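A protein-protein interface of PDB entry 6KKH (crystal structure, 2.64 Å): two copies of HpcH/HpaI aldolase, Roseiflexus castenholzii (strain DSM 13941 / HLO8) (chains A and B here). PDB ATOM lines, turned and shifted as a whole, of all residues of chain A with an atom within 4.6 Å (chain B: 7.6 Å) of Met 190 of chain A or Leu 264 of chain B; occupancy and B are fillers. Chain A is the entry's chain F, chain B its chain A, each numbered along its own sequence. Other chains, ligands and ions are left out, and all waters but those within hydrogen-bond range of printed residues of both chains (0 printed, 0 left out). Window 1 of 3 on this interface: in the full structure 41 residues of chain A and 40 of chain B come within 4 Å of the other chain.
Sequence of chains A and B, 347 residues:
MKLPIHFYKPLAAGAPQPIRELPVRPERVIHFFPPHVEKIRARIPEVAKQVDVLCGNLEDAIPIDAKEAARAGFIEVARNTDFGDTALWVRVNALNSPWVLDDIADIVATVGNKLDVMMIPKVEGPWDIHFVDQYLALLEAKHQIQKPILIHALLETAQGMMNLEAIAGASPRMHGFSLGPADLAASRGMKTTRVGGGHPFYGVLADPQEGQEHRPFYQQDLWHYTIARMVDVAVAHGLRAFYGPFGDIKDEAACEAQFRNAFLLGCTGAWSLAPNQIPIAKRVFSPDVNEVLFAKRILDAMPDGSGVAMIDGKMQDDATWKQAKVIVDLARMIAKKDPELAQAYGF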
ATOM      1  N   ALA A 185      -2.484  -9.667 -24.945  1.00  0.00           N
ATOM      2  CA  ALA A 185      -1.315 -10.363 -24.394  1.00  0.00           C
ATOM      3  C   ALA A 185      -1.226 -10.137 -22.877  1.00  0.00           C
ATOM      4  O   ALA A 185      -0.813 -11.037 -22.146  1.00  0.00           O
ATOM      5  CB  ALA A 185      -0.062  -9.897 -25.091  1.00  0.00           C
ATOM      6  N   ARG A 188      -4.227 -12.247 -21.394  1.00  0.00           N
ATOM      7  CA  ARG A 188      -3.915 -13.687 -21.425  1.00  0.00           C
ATOM      8  C   ARG A 188      -2.753 -14.005 -20.476  1.00  0.00           C
ATOM      9  O   ARG A 188      -2.650 -15.124 -19.972  1.00  0.00           O
ATOM     10  CB  ARG A 188      -3.540 -14.145 -22.838  1.00  0.00           C
ATOM     11  CG  ARG A 188      -4.720 -14.314 -23.781  1.00  0.00           C
ATOM     12  CD  ARG A 188      -4.267 -14.475 -25.217  1.00  0.00           C
ATOM     13  NE  ARG A 188      -5.379 -14.739 -26.116  1.00  0.00           N
ATOM     14  CZ  ARG A 188      -5.246 -15.065 -27.396  1.00  0.00           C
ATOM     15  NH1 ARG A 188      -4.067 -14.965 -27.981  1.00  0.00           N
ATOM     16  NH2 ARG A 188      -6.288 -15.504 -28.083  1.00  0.00           N
ATOM     17  N   GLY A 189      -1.879 -13.025 -20.261  1.00  0.00           N
ATOM     18  CA  GLY A 189      -0.598 -13.253 -19.609  1.00  0.00           C
ATOM     19  C   GLY A 189       0.433 -13.794 -20.585  1.00  0.00           C
ATOM     20  O   GLY A 189       1.389 -14.423 -20.164  1.00  0.00           O
ATOM     21  N   MET A 190       0.244 -13.576 -21.889  1.00  0.00           N
ATOM     22  CA  MET A 190       1.296 -13.892 -22.859  1.00  0.00           C
ATOM     23  C   MET A 190       2.559 -13.135 -22.434  1.00  0.00           C
ATOM     24  O   MET A 190       2.484 -11.938 -22.141  1.00  0.00           O
ATOM     25  CB  MET A 190       0.912 -13.473 -24.285  1.00  0.00           C
ATOM     26  CG  MET A 190      -0.194 -14.304 -24.906  1.00  0.00           C
ATOM     27  SD  MET A 190      -0.816 -13.628 -26.481  1.00  0.00           S
ATOM     28  CE  MET A 190      -0.096 -14.763 -27.663  1.00  0.00           C
ATOM     29  N   LYS A 191       3.701 -13.816 -22.367  1.00  0.00           N
ATOM     30  CA  LYS A 191       4.913 -13.194 -21.805  1.00  0.00           C
ATOM     31  C   LYS A 191       5.736 -12.551 -22.929  1.00  0.00           C
ATOM     32  O   LYS A 191       6.807 -13.022 -23.306  1.00  0.00           O
ATOM     33  CB  LYS A 191       5.708 -14.198 -20.963  1.00  0.00           C
ATOM     34  CG  LYS A 191       5.380 -14.164 -19.476  1.00  0.00           C
ATOM     35  CD  LYS A 191       4.264 -15.100 -19.065  1.00  0.00           C
ATOM     36  CE  LYS A 191       3.518 -14.629 -17.833  1.00  0.00           C
ATOM     37  NZ  LYS A 191       2.250 -15.375 -17.660  1.00  0.00           N
ATOM     38  N   THR A 192       5.184 -11.459 -23.451  1.00  0.00           N
ATOM     39  CA  THR A 192       5.874 -10.539 -24.341  1.00  0.00           C
ATOM     40  C   THR A 192       5.426  -9.119 -23.982  1.00  0.00           C
ATOM     41  O   THR A 192       4.298  -8.931 -23.525  1.00  0.00           O
ATOM     42  CB  THR A 192       5.587 -10.846 -25.817  1.00  0.00           C
ATOM     43  OG1 THR A 192       4.421 -10.120 -26.208  1.00  0.00           O
ATOM     44  CG2 THR A 192       5.383 -12.319 -26.100  1.00  0.00           C
ATOM     45  N   HIS A 199       7.777 -13.842 -32.282  1.00  0.00           N
ATOM     46  CA  HIS A 199       8.633 -13.785 -31.101  1.00  0.00           C
ATOM     47  C   HIS A 199       9.732 -14.833 -31.284  1.00  0.00           C
ATOM     48  O   HIS A 199       9.449 -15.932 -31.757  1.00  0.00           O
ATOM     49  CB  HIS A 199       7.821 -13.972 -29.812  1.00  0.00           C
ATOM     50  CG  HIS A 199       8.562 -13.615 -28.566  1.00  0.00           C
ATOM     51  ND1 HIS A 199       9.615 -14.375 -28.085  1.00  0.00           N
ATOM     52  CD2 HIS A 199       8.404 -12.593 -27.693  1.00  0.00           C
ATOM     53  CE1 HIS A 199      10.075 -13.830 -26.974  1.00  0.00           C
ATOM     54  NE2 HIS A 199       9.345 -12.738 -26.706  1.00  0.00           N
ATOM     55  N   PHE A 201      11.537 -16.684 -29.239  1.00  0.00           N
ATOM     56  CA  PHE A 201      11.582 -17.850 -28.354  1.00  0.00           C
ATOM     57  C   PHE A 201      10.369 -18.772 -28.570  1.00  0.00           C
ATOM     58  O   PHE A 201      10.331 -19.875 -28.003  1.00  0.00           O
ATOM     59  CB  PHE A 201      11.678 -17.403 -26.891  1.00  0.00           C
ATOM     60  CG  PHE A 201      12.926 -16.637 -26.517  1.00  0.00           C
ATOM     61  CD1 PHE A 201      14.160 -16.945 -27.077  1.00  0.00           C
ATOM     62  CD2 PHE A 201      12.871 -15.624 -25.570  1.00  0.00           C
ATOM     63  CE1 PHE A 201      15.301 -16.242 -26.718  1.00  0.00           C
ATOM     64  CE2 PHE A 201      14.012 -14.923 -25.211  1.00  0.00           C
ATOM     65  CZ  PHE A 201      15.225 -15.234 -25.785  1.00  0.00           C
ATOM     66  N   TYR A 202       9.385 -18.357 -29.367  1.00  0.00           N
ATOM     67  CA  TYR A 202       8.274 -19.243 -29.677  1.00  0.00           C
ATOM     68  C   TYR A 202       8.597 -20.019 -30.960  1.00  0.00           C
ATOM     69  O   TYR A 202       8.440 -19.508 -32.078  1.00  0.00           O
ATOM     70  CB  TYR A 202       6.948 -18.482 -29.785  1.00  0.00           C
ATOM     71  CG  TYR A 202       5.749 -19.372 -30.008  1.00  0.00           C
ATOM     72  CD1 TYR A 202       5.526 -20.479 -29.204  1.00  0.00           C
ATOM     73  CD2 TYR A 202       4.840 -19.131 -31.028  1.00  0.00           C
ATOM     74  CE1 TYR A 202       4.439 -21.316 -29.402  1.00  0.00           C
ATOM     75  CE2 TYR A 202       3.742 -19.953 -31.236  1.00  0.00           C
ATOM     76  CZ  TYR A 202       3.538 -21.053 -30.420  1.00  0.00           C
ATOM     77  OH  TYR A 202       2.470 -21.886 -30.603  1.00  0.00           O
ATOM     78  N   LEU A 222       2.560 -16.772 -33.002  1.00  0.00           N
ATOM     79  CA  LEU A 222       1.848 -16.628 -31.715  1.00  0.00           C
ATOM     80  C   LEU A 222       0.333 -16.500 -31.922  1.00  0.00           C
ATOM     81  O   LEU A 222      -0.415 -16.918 -31.049  1.00  0.00           O
ATOM     82  CB  LEU A 222       2.357 -15.387 -30.970  1.00  0.00           C
ATOM     83  CG  LEU A 222       3.637 -15.544 -30.148  1.00  0.00           C
ATOM     84  CD1 LEU A 222       4.042 -14.205 -29.547  1.00  0.00           C
ATOM     85  CD2 LEU A 222       3.470 -16.577 -29.040  1.00  0.00           C
ATOM     86  N   TRP A 223      -0.108 -15.902 -33.032  1.00  0.00           N
ATOM     87  CA  TRP A 223      -1.497 -15.435 -33.175  1.00  0.00           C
ATOM     88  C   TRP A 223      -2.293 -16.276 -34.181  1.00  0.00           C
ATOM     89  O   TRP A 223      -3.314 -15.802 -34.661  1.00  0.00           O
ATOM     90  CB  TRP A 223      -1.525 -13.963 -33.601  1.00  0.00           C
ATOM     91  CG  TRP A 223      -0.690 -13.054 -32.757  1.00  0.00           C
ATOM     92  CD1 TRP A 223       0.549 -12.566 -33.053  1.00  0.00           C
ATOM     93  CD2 TRP A 223      -1.036 -12.514 -31.471  1.00  0.00           C
ATOM     94  NE1 TRP A 223       0.999 -11.765 -32.038  1.00  0.00           N
ATOM     95  CE2 TRP A 223       0.049 -11.716 -31.054  1.00  0.00           C
ATOM     96  CE3 TRP A 223      -2.150 -12.631 -30.633  1.00  0.00           C
ATOM     97  CZ2 TRP A 223       0.047 -11.034 -29.841  1.00  0.00           C
ATOM     98  CZ3 TRP A 223      -2.152 -11.953 -29.431  1.00  0.00           C
ATOM     99  CH2 TRP A 223      -1.066 -11.169 -29.043  1.00  0.00           C
ATOM    100  N   HIS B 224      -0.272 -25.987 -30.646  1.00  0.00           N
ATOM    101  CA  HIS B 224      -0.588 -24.551 -30.657  1.00  0.00           C
ATOM    102  C   HIS B 224      -2.065 -24.315 -30.303  1.00  0.00           C
ATOM    103  O   HIS B 224      -2.359 -23.550 -29.388  1.00  0.00           O
ATOM    104  CB  HIS B 224      -0.214 -23.922 -32.006  1.00  0.00           C
ATOM    105  CG  HIS B 224      -0.661 -22.507 -32.133  1.00  0.00           C
ATOM    106  ND1 HIS B 224      -0.113 -21.492 -31.370  1.00  0.00           N
ATOM    107  CD2 HIS B 224      -1.623 -21.939 -32.893  1.00  0.00           C
ATOM    108  CE1 HIS B 224      -0.711 -20.356 -31.663  1.00  0.00           C
ATOM    109  NE2 HIS B 224      -1.638 -20.604 -32.596  1.00  0.00           N
ATOM    110  N   ILE B 227      -2.996 -25.439 -26.695  1.00  0.00           N
ATOM    111  CA  ILE B 227      -2.462 -24.590 -25.615  1.00  0.00           C
ATOM    112  C   ILE B 227      -3.191 -23.241 -25.638  1.00  0.00           C
ATOM    113  O   ILE B 227      -3.565 -22.711 -24.588  1.00  0.00           O
ATOM    114  CB  ILE B 227      -0.933 -24.394 -25.710  1.00  0.00           C
ATOM    115  CG1 ILE B 227      -0.166 -25.720 -25.731  1.00  0.00           C
ATOM    116  CG2 ILE B 227      -0.454 -23.481 -24.584  1.00  0.00           C
ATOM    117  CD1 ILE B 227       0.245 -26.224 -24.374  1.00  0.00           C
ATOM    118  N   ALA B 228      -3.359 -22.688 -26.834  1.00  0.00           N
ATOM    119  CA  ALA B 228      -4.001 -21.387 -26.997  1.00  0.00           C
ATOM    120  C   ALA B 228      -5.420 -21.450 -26.417  1.00  0.00           C
ATOM    121  O   ALA B 228      -5.856 -20.518 -25.732  1.00  0.00           O
ATOM    122  CB  ALA B 228      -4.008 -20.994 -28.455  1.00  0.00           C
ATOM    123  N   VAL B 231      -5.444 -21.806 -22.515  1.00  0.00           N
ATOM    124  CA  VAL B 231      -5.072 -20.551 -21.853  1.00  0.00           C
ATOM    125  C   VAL B 231      -6.265 -19.579 -21.865  1.00  0.00           C
ATOM    126  O   VAL B 231      -6.562 -18.946 -20.837  1.00  0.00           O
ATOM    127  CB  VAL B 231      -3.811 -19.933 -22.496  1.00  0.00           C
ATOM    128  CG1 VAL B 231      -3.558 -18.505 -22.033  1.00  0.00           C
ATOM    129  CG2 VAL B 231      -2.578 -20.784 -22.238  1.00  0.00           C
ATOM    130  N   ASP B 232      -6.961 -19.446 -22.991  1.00  0.00           N
ATOM    131  CA  ASP B 232      -8.079 -18.486 -23.055  1.00  0.00           C
ATOM    132  C   ASP B 232      -9.158 -18.894 -22.038  1.00  0.00           C
ATOM    133  O   ASP B 232      -9.585 -18.081 -21.206  1.00  0.00           O
ATOM    134  CB  ASP B 232      -8.635 -18.342 -24.479  1.00  0.00           C
ATOM    135  CG  ASP B 232      -8.018 -17.218 -25.310  1.00  0.00           C
ATOM    136  OD1 ASP B 232      -7.246 -16.412 -24.750  1.00  0.00           O
ATOM    137  OD2 ASP B 232      -8.322 -17.149 -26.522  1.00  0.00           O
ATOM    138  N   VAL B 235      -7.942 -18.523 -18.307  1.00  0.00           N
ATOM    139  CA  VAL B 235      -7.655 -17.159 -17.856  1.00  0.00           C
ATOM    140  C   VAL B 235      -8.962 -16.362 -17.789  1.00  0.00           C
ATOM    141  O   VAL B 235      -9.134 -15.559 -16.879  1.00  0.00           O
ATOM    142  CB  VAL B 235      -6.610 -16.474 -18.759  1.00  0.00           C
ATOM    143  CG1 VAL B 235      -6.433 -15.004 -18.415  1.00  0.00           C
ATOM    144  CG2 VAL B 235      -5.271 -17.193 -18.708  1.00  0.00           C
ATOM    145  N   ALA B 257      12.685 -25.917 -24.766  1.00  0.00           N
ATOM    146  CA  ALA B 257      12.012 -25.381 -25.943  1.00  0.00           C
ATOM    147  C   ALA B 257      10.491 -25.491 -25.777  1.00  0.00           C
ATOM    148  O   ALA B 257       9.749 -24.533 -26.040  1.00  0.00           O
ATOM    149  CB  ALA B 257      12.478 -26.124 -27.171  1.00  0.00           C
ATOM    150  N   GLN B 258      10.046 -26.665 -25.330  1.00  0.00           N
ATOM    151  CA  GLN B 258       8.629 -26.960 -25.182  1.00  0.00           C
ATOM    152  C   GLN B 258       8.048 -26.150 -24.015  1.00  0.00           C
ATOM    153  O   GLN B 258       7.001 -25.514 -24.156  1.00  0.00           O
ATOM    154  CB  GLN B 258       8.430 -28.458 -24.962  1.00  0.00           C
ATOM    155  CG  GLN B 258       7.062 -28.955 -25.399  1.00  0.00           C
ATOM    156  CD  GLN B 258       6.946 -29.140 -26.892  1.00  0.00           C
ATOM    157  OE1 GLN B 258       7.809 -28.732 -27.666  1.00  0.00           O
ATOM    158  NE2 GLN B 258       5.857 -29.758 -27.313  1.00  0.00           N
ATOM    159  N   PHE B 259       8.733 -26.169 -22.873  1.00  0.00           N
ATOM    160  CA  PHE B 259       8.304 -25.404 -21.691  1.00  0.00           C
ATOM    161  C   PHE B 259       8.224 -23.908 -22.028  1.00  0.00           C
ATOM    162  O   PHE B 259       7.317 -23.218 -21.573  1.00  0.00           O
ATOM    163  CB  PHE B 259       9.260 -25.643 -20.517  1.00  0.00           C
ATOM    164  CG  PHE B 259       9.100 -26.946 -19.768  1.00  0.00           C
ATOM    165  CD1 PHE B 259       8.235 -27.942 -20.201  1.00  0.00           C
ATOM    166  CD2 PHE B 259       9.848 -27.189 -18.625  1.00  0.00           C
ATOM    167  CE1 PHE B 259       8.113 -29.133 -19.502  1.00  0.00           C
ATOM    168  CE2 PHE B 259       9.730 -28.385 -17.932  1.00  0.00           C
ATOM    169  CZ  PHE B 259       8.861 -29.355 -18.372  1.00  0.00           C
ATOM    170  N   ARG B 260       9.170 -23.416 -22.822  1.00  0.00           N
ATOM    171  CA  ARG B 260       9.283 -21.984 -23.105  1.00  0.00           C
ATOM    172  C   ARG B 260       8.103 -21.546 -23.975  1.00  0.00           C
ATOM    173  O   ARG B 260       7.530 -20.483 -23.749  1.00  0.00           O
ATOM    174  CB  ARG B 260      10.619 -21.690 -23.797  1.00  0.00           C
ATOM    175  CG  ARG B 260      11.089 -20.245 -23.702  1.00  0.00           C
ATOM    176  CD  ARG B 260      12.537 -20.114 -24.145  1.00  0.00           C
ATOM    177  NE  ARG B 260      12.707 -20.641 -25.494  1.00  0.00           N
ATOM    178  CZ  ARG B 260      13.813 -21.217 -25.953  1.00  0.00           C
ATOM    179  NH1 ARG B 260      14.892 -21.285 -25.191  1.00  0.00           N
ATOM    180  NH2 ARG B 260      13.831 -21.731 -27.171  1.00  0.00           N
ATOM    181  N   ASN B 261       7.756 -22.374 -24.961  1.00  0.00           N
ATOM    182  CA  ASN B 261       6.599 -22.117 -25.818  1.00  0.00           C
ATOM    183  C   ASN B 261       5.353 -21.922 -24.942  1.00  0.00           C
ATOM    184  O   ASN B 261       4.572 -20.989 -25.149  1.00  0.00           O
ATOM    185  CB  ASN B 261       6.365 -23.246 -26.822  1.00  0.00           C
ATOM    186  CG  ASN B 261       7.337 -23.265 -27.984  1.00  0.00           C
ATOM    187  OD1 ASN B 261       8.080 -22.317 -28.208  1.00  0.00           O
ATOM    188  ND2 ASN B 261       7.325 -24.346 -28.746  1.00  0.00           N
ATOM    189  N   ALA B 262       5.189 -22.794 -23.951  1.00  0.00           N
ATOM    190  CA  ALA B 262       4.025 -22.750 -23.083  1.00  0.00           C
ATOM    191  C   ALA B 262       4.056 -21.485 -22.214  1.00  0.00           C
ATOM    192  O   ALA B 262       3.021 -20.847 -22.001  1.00  0.00           O
ATOM    193  CB  ALA B 262       3.960 -24.005 -22.246  1.00  0.00           C
ATOM    194  N   PHE B 263       5.228 -21.118 -21.714  1.00  0.00           N
ATOM    195  CA  PHE B 263       5.350 -19.928 -20.873  1.00  0.00           C
ATOM    196  C   PHE B 263       4.895 -18.690 -21.652  1.00  0.00           C
ATOM    197  O   PHE B 263       4.163 -17.860 -21.122  1.00  0.00           O
ATOM    198  CB  PHE B 263       6.788 -19.764 -20.378  1.00  0.00           C
ATOM    199  CG  PHE B 263       7.032 -18.548 -19.522  1.00  0.00           C
ATOM    200  CD1 PHE B 263       6.459 -18.440 -18.264  1.00  0.00           C
ATOM    201  CD2 PHE B 263       7.831 -17.508 -19.974  1.00  0.00           C
ATOM    202  CE1 PHE B 263       6.688 -17.325 -17.472  1.00  0.00           C
ATOM    203  CE2 PHE B 263       8.058 -16.394 -19.183  1.00  0.00           C
ATOM    204  CZ  PHE B 263       7.491 -16.306 -17.931  1.00  0.00           C
ATOM    205  N   LEU B 264       5.307 -18.601 -22.913  1.00  0.00           N
ATOM    206  CA  LEU B 264       5.049 -17.419 -23.740  1.00  0.00           C
ATOM    207  C   LEU B 264       3.565 -17.319 -24.119  1.00  0.00           C
ATOM    208  O   LEU B 264       3.022 -16.218 -24.184  1.00  0.00           O
ATOM    209  CB  LEU B 264       5.928 -17.488 -24.993  1.00  0.00           C
ATOM    210  CG  LEU B 264       7.427 -17.326 -24.743  1.00  0.00           C
ATOM    211  CD1 LEU B 264       8.239 -17.758 -25.958  1.00  0.00           C
ATOM    212  CD2 LEU B 264       7.761 -15.891 -24.353  1.00  0.00           C
ATOM    213  N   LEU B 265       2.927 -18.447 -24.408  1.00  0.00           N
ATOM    214  CA  LEU B 265       1.510 -18.448 -24.743  1.00  0.00           C
ATOM    215  C   LEU B 265       0.681 -18.130 -23.494  1.00  0.00           C
ATOM    216  O   LEU B 265      -0.453 -17.663 -23.627  1.00  0.00           O
ATOM    217  CB  LEU B 265       1.108 -19.809 -25.322  1.00  0.00           C
ATOM    218  CG  LEU B 265       1.478 -20.044 -26.783  1.00  0.00           C
ATOM    219  CD1 LEU B 265       0.994 -21.412 -27.239  1.00  0.00           C
ATOM    220  CD2 LEU B 265       0.911 -18.948 -27.673  1.00  0.00           C
ATOM    221  N   GLY B 266       1.227 -18.402 -22.307  1.00  0.00           N
ATOM    222  CA  GLY B 266       0.648 -17.891 -21.055  1.00  0.00           C
ATOM    223  C   GLY B 266       0.424 -18.953 -19.980  1.00  0.00           C
ATOM    224  O   GLY B 266      -0.328 -18.694 -19.043  1.00  0.00           O
ATOM    225  N   CYS B 267       1.071 -20.118 -20.069  1.00  0.00           N
ATOM    226  CA  CYS B 267       0.999 -21.116 -18.997  1.00  0.00           C
ATOM    227  C   CYS B 267       1.848 -20.652 -17.811  1.00  0.00           C
ATOM    228  O   CYS B 267       2.786 -19.884 -17.978  1.00  0.00           O
ATOM    229  CB  CYS B 267       1.465 -22.487 -19.468  1.00  0.00           C
ATOM    230  SG  CYS B 267       0.446 -23.174 -20.800  1.00  0.00           S
ATOM    231  N   VAL B 284      12.530 -21.523 -16.818  1.00  0.00           N
ATOM    232  CA  VAL B 284      11.745 -21.180 -18.011  1.00  0.00           C
ATOM    233  C   VAL B 284      10.481 -20.407 -17.622  1.00  0.00           C
ATOM    234  O   VAL B 284      10.064 -19.515 -18.353  1.00  0.00           O
ATOM    235  CB  VAL B 284      11.402 -22.441 -18.828  1.00  0.00           C
ATOM    236  CG1 VAL B 284      10.249 -22.212 -19.790  1.00  0.00           C
ATOM    237  CG2 VAL B 284      12.617 -22.960 -19.582  1.00  0.00           C
ATOM    238  N   PHE B 285       9.871 -20.745 -16.493  1.00  0.00           N
ATOM    239  CA  PHE B 285       8.593 -20.137 -16.100  1.00  0.00           C
ATOM    240  C   PHE B 285       8.829 -18.943 -15.166  1.00  0.00           C
ATOM    241  O   PHE B 285       7.872 -18.383 -14.631  1.00  0.00           O
ATOM    242  CB  PHE B 285       7.663 -21.205 -15.518  1.00  0.00           C
ATOM    243  CG  PHE B 285       7.117 -22.134 -16.570  1.00  0.00           C
ATOM    244  CD1 PHE B 285       5.993 -21.792 -17.303  1.00  0.00           C
ATOM    245  CD2 PHE B 285       7.749 -23.330 -16.861  1.00  0.00           C
ATOM    246  CE1 PHE B 285       5.507 -22.630 -18.296  1.00  0.00           C
ATOM    247  CE2 PHE B 285       7.256 -24.170 -17.850  1.00  0.00           C
ATOM    248  CZ  PHE B 285       6.137 -23.819 -18.565  1.00  0.00           C
ATOM    249  N   GLU B 291      13.895  -9.357 -20.647  1.00  0.00           N
ATOM    250  CA  GLU B 291      12.528  -8.850 -20.808  1.00  0.00           C
ATOM    251  C   GLU B 291      12.123  -8.019 -19.582  1.00  0.00           C
ATOM    252  O   GLU B 291      11.341  -7.081 -19.712  1.00  0.00           O
ATOM    253  CB  GLU B 291      11.559 -10.010 -21.060  1.00  0.00           C
ATOM    254  CG  GLU B 291      11.803 -10.732 -22.377  1.00  0.00           C
ATOM    255  CD  GLU B 291      10.560 -11.331 -23.019  1.00  0.00           C
ATOM    256  OE1 GLU B 291      10.082 -12.374 -22.525  1.00  0.00           O
ATOM    257  OE2 GLU B 291      10.070 -10.753 -24.010  1.00  0.00           O
ATOM    258  N   GLN B 323       1.279  -4.973 -20.006  1.00  0.00           N
ATOM    259  CA  GLN B 323       2.147  -6.095 -20.402  1.00  0.00           C
ATOM    260  C   GLN B 323       3.405  -6.120 -19.523  1.00  0.00           C
ATOM    261  O   GLN B 323       3.854  -7.183 -19.098  1.00  0.00           O
ATOM    262  CB  GLN B 323       2.537  -5.987 -21.878  1.00  0.00           C
ATOM    263  CG  GLN B 323       1.383  -6.248 -22.832  1.00  0.00           C
ATOM    264  CD  GLN B 323       1.827  -6.330 -24.273  1.00  0.00           C
ATOM    265  OE1 GLN B 323       2.236  -7.380 -24.762  1.00  0.00           O
ATOM    266  NE2 GLN B 323       1.724  -5.215 -24.976  1.00  0.00           N
ATOM    267  N   VAL B 326       2.718  -7.185 -15.799  1.00  0.00           N
ATOM    268  CA  VAL B 326       2.609  -8.652 -15.672  1.00  0.00           C
ATOM    269  C   VAL B 326       4.006  -9.253 -15.449  1.00  0.00           C
ATOM    270  O   VAL B 326       4.218  -9.987 -14.486  1.00  0.00           O
ATOM    271  CB  VAL B 326       1.919  -9.278 -16.903  1.00  0.00           C
ATOM    272  CG1 VAL B 326       2.215 -10.766 -17.053  1.00  0.00           C
ATOM    273  CG2 VAL B 326       0.418  -9.036 -16.882  1.00  0.00           C
ATOM    274  N   ILE B 327       4.942  -8.936 -16.340  1.00  0.00           N
ATOM    275  CA  ILE B 327       6.285  -9.527 -16.314  1.00  0.00           C
ATOM    276  C   ILE B 327       7.052  -9.049 -15.070  1.00  0.00           C
ATOM    277  O   ILE B 327       7.839  -9.818 -14.510  1.00  0.00           O
ATOM    278  CB  ILE B 327       7.031  -9.224 -17.633  1.00  0.00           C
ATOM    279  CG1 ILE B 327       6.472 -10.067 -18.784  1.00  0.00           C
ATOM    280  CG2 ILE B 327       8.536  -9.411 -17.483  1.00  0.00           C
ATOM    281  CD1 ILE B 327       6.835  -9.562 -20.164  1.00  0.00           C
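No position is printed for both chains. Of the 20 pairs that touch across the chains among the printed residues, none has its exchanged pair printed and touching as well.
CB of Ala 185 of chain A touches OE1 of Gln 323 of chain B (3.4 Å). Arg 188 of chain A touches Val 235 of chain B (O to CG2, 3.6 Å). Met 190 of chain A touches Leu 264 of chain B (CA to O, 3.2 Å). CG of Met 190 of chain A touches O of Leu 265 of chain B (3.6 Å). CG of Lys 191 of chain A touches CZ of Phe 263 of chain B (3.4 Å). Phe 201 of chain A touches Arg 260 of chain B. Asn 261 of chain B touches Tyr 202 of chain A (OD1 to CD1, 3.3 Å). CD1 of Leu 265 of chain B touches OH of Tyr 202 of chain A, at 3.7 Å. His 224 of chain B touches Leu 222 of chain A. CD2 of Leu 222 of chain A touches CD2 of Leu 265 of chain B, at 3.7 Å.
The backbone carbonyl oxygen (O) of Ala 185 of chain A is in hydrogen-bond range of the backbone NH (N) of Met 190 of chain A. A ring nitrogen (ND1) of His 199 of chain A sits at hydrogen-bond distance from the backbone NH (N) of Phe 201 of chain A (3.2 Å). The side-chain amino group of Lys 191 of chain A is in hydrogen-bond range of the backbone carbonyl oxygen of Gly 189 of chain A (2.8 Å).
The side-chain carboxylate of Glu 291 of chain B sits at hydrogen-bond distance from a ring nitrogen (NE2) of His 199 of chain A (3.4 Å). OD1 of Asn 261 of chain B lies close to O of Phe 201 of chain A, 3.3 Å away. The backbone carbonyl oxygen (O) of Leu 264 of chain B lies within hydrogen-bond range of the backbone NH (N) of Lys 191 of chain A (3.1 Å). O of Lys 191 of chain A sits close to OE1 of Glu 291 of chain B, 3.4 Å away. The side-chain amide oxygen (OE1) of Gln 323 of chain B sits close to the backbone carbonyl oxygen (O) of Thr 192 of chain A. The side-chain carboxylate (OD1) of Asp 232 of chain B is in salt-bridge range of the guanidinium group (NE) of Arg 188 of chain A (2.9 Å). ND1 of His 224 of chain B lies within hydrogen-bond range of OH of Tyr 202 of chain A, at 2.7 Å.
Gly 189 of chain A touches one residue of chain B. Of chain B, only Leu 264 and Leu 265 come within 4 Å of Met 190 of chain A. Printed residues of chain B within 4 Å of Lys 191 of chain A: Phe 263, Leu 264 and Glu 291. Of the printed residues of chain B, Thr 192 of chain A touches Gln 323 (2.9 Å). Ile 227 of chain B touches none of the printed residues of chain A. Of chain A, only Met 190, Lys 191, Phe 201 and Tyr 202 come within 4 Å of Leu 264 of chain B. Cys 267 of chain B touches none of the printed residues of chain A. Of the printed residues of chain A, Glu 291 of chain B touches Lys 191 and His 199. The nearest printed residue of chain A that does not touch Phe 263 of chain B is Gly 189 of chain A (4.5 Å).
Printed residues of chain A that touch a printed residue of chain B: Ala 185, Arg 188, Gly 189, Met 190, Lys 191, Thr 192, His 199, Phe 201, Tyr 202 and Leu 222. Hydrophobic or aromatic side chains of chain A that line the printed part of chain B: Ala 185, Met 190, His 199, Phe 201, Tyr 202 and Leu 222. Of the 23 printed residues of chain B, 11 touch a printed residue of chain A. Printed residues of chain B that touch a printed residue of chain A: His 224, Asp 232, Val 235, Arg 260, Asn 261, Phe 263, Leu 264, Leu 265, Gly 266, Glu 291 and Gln 323.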
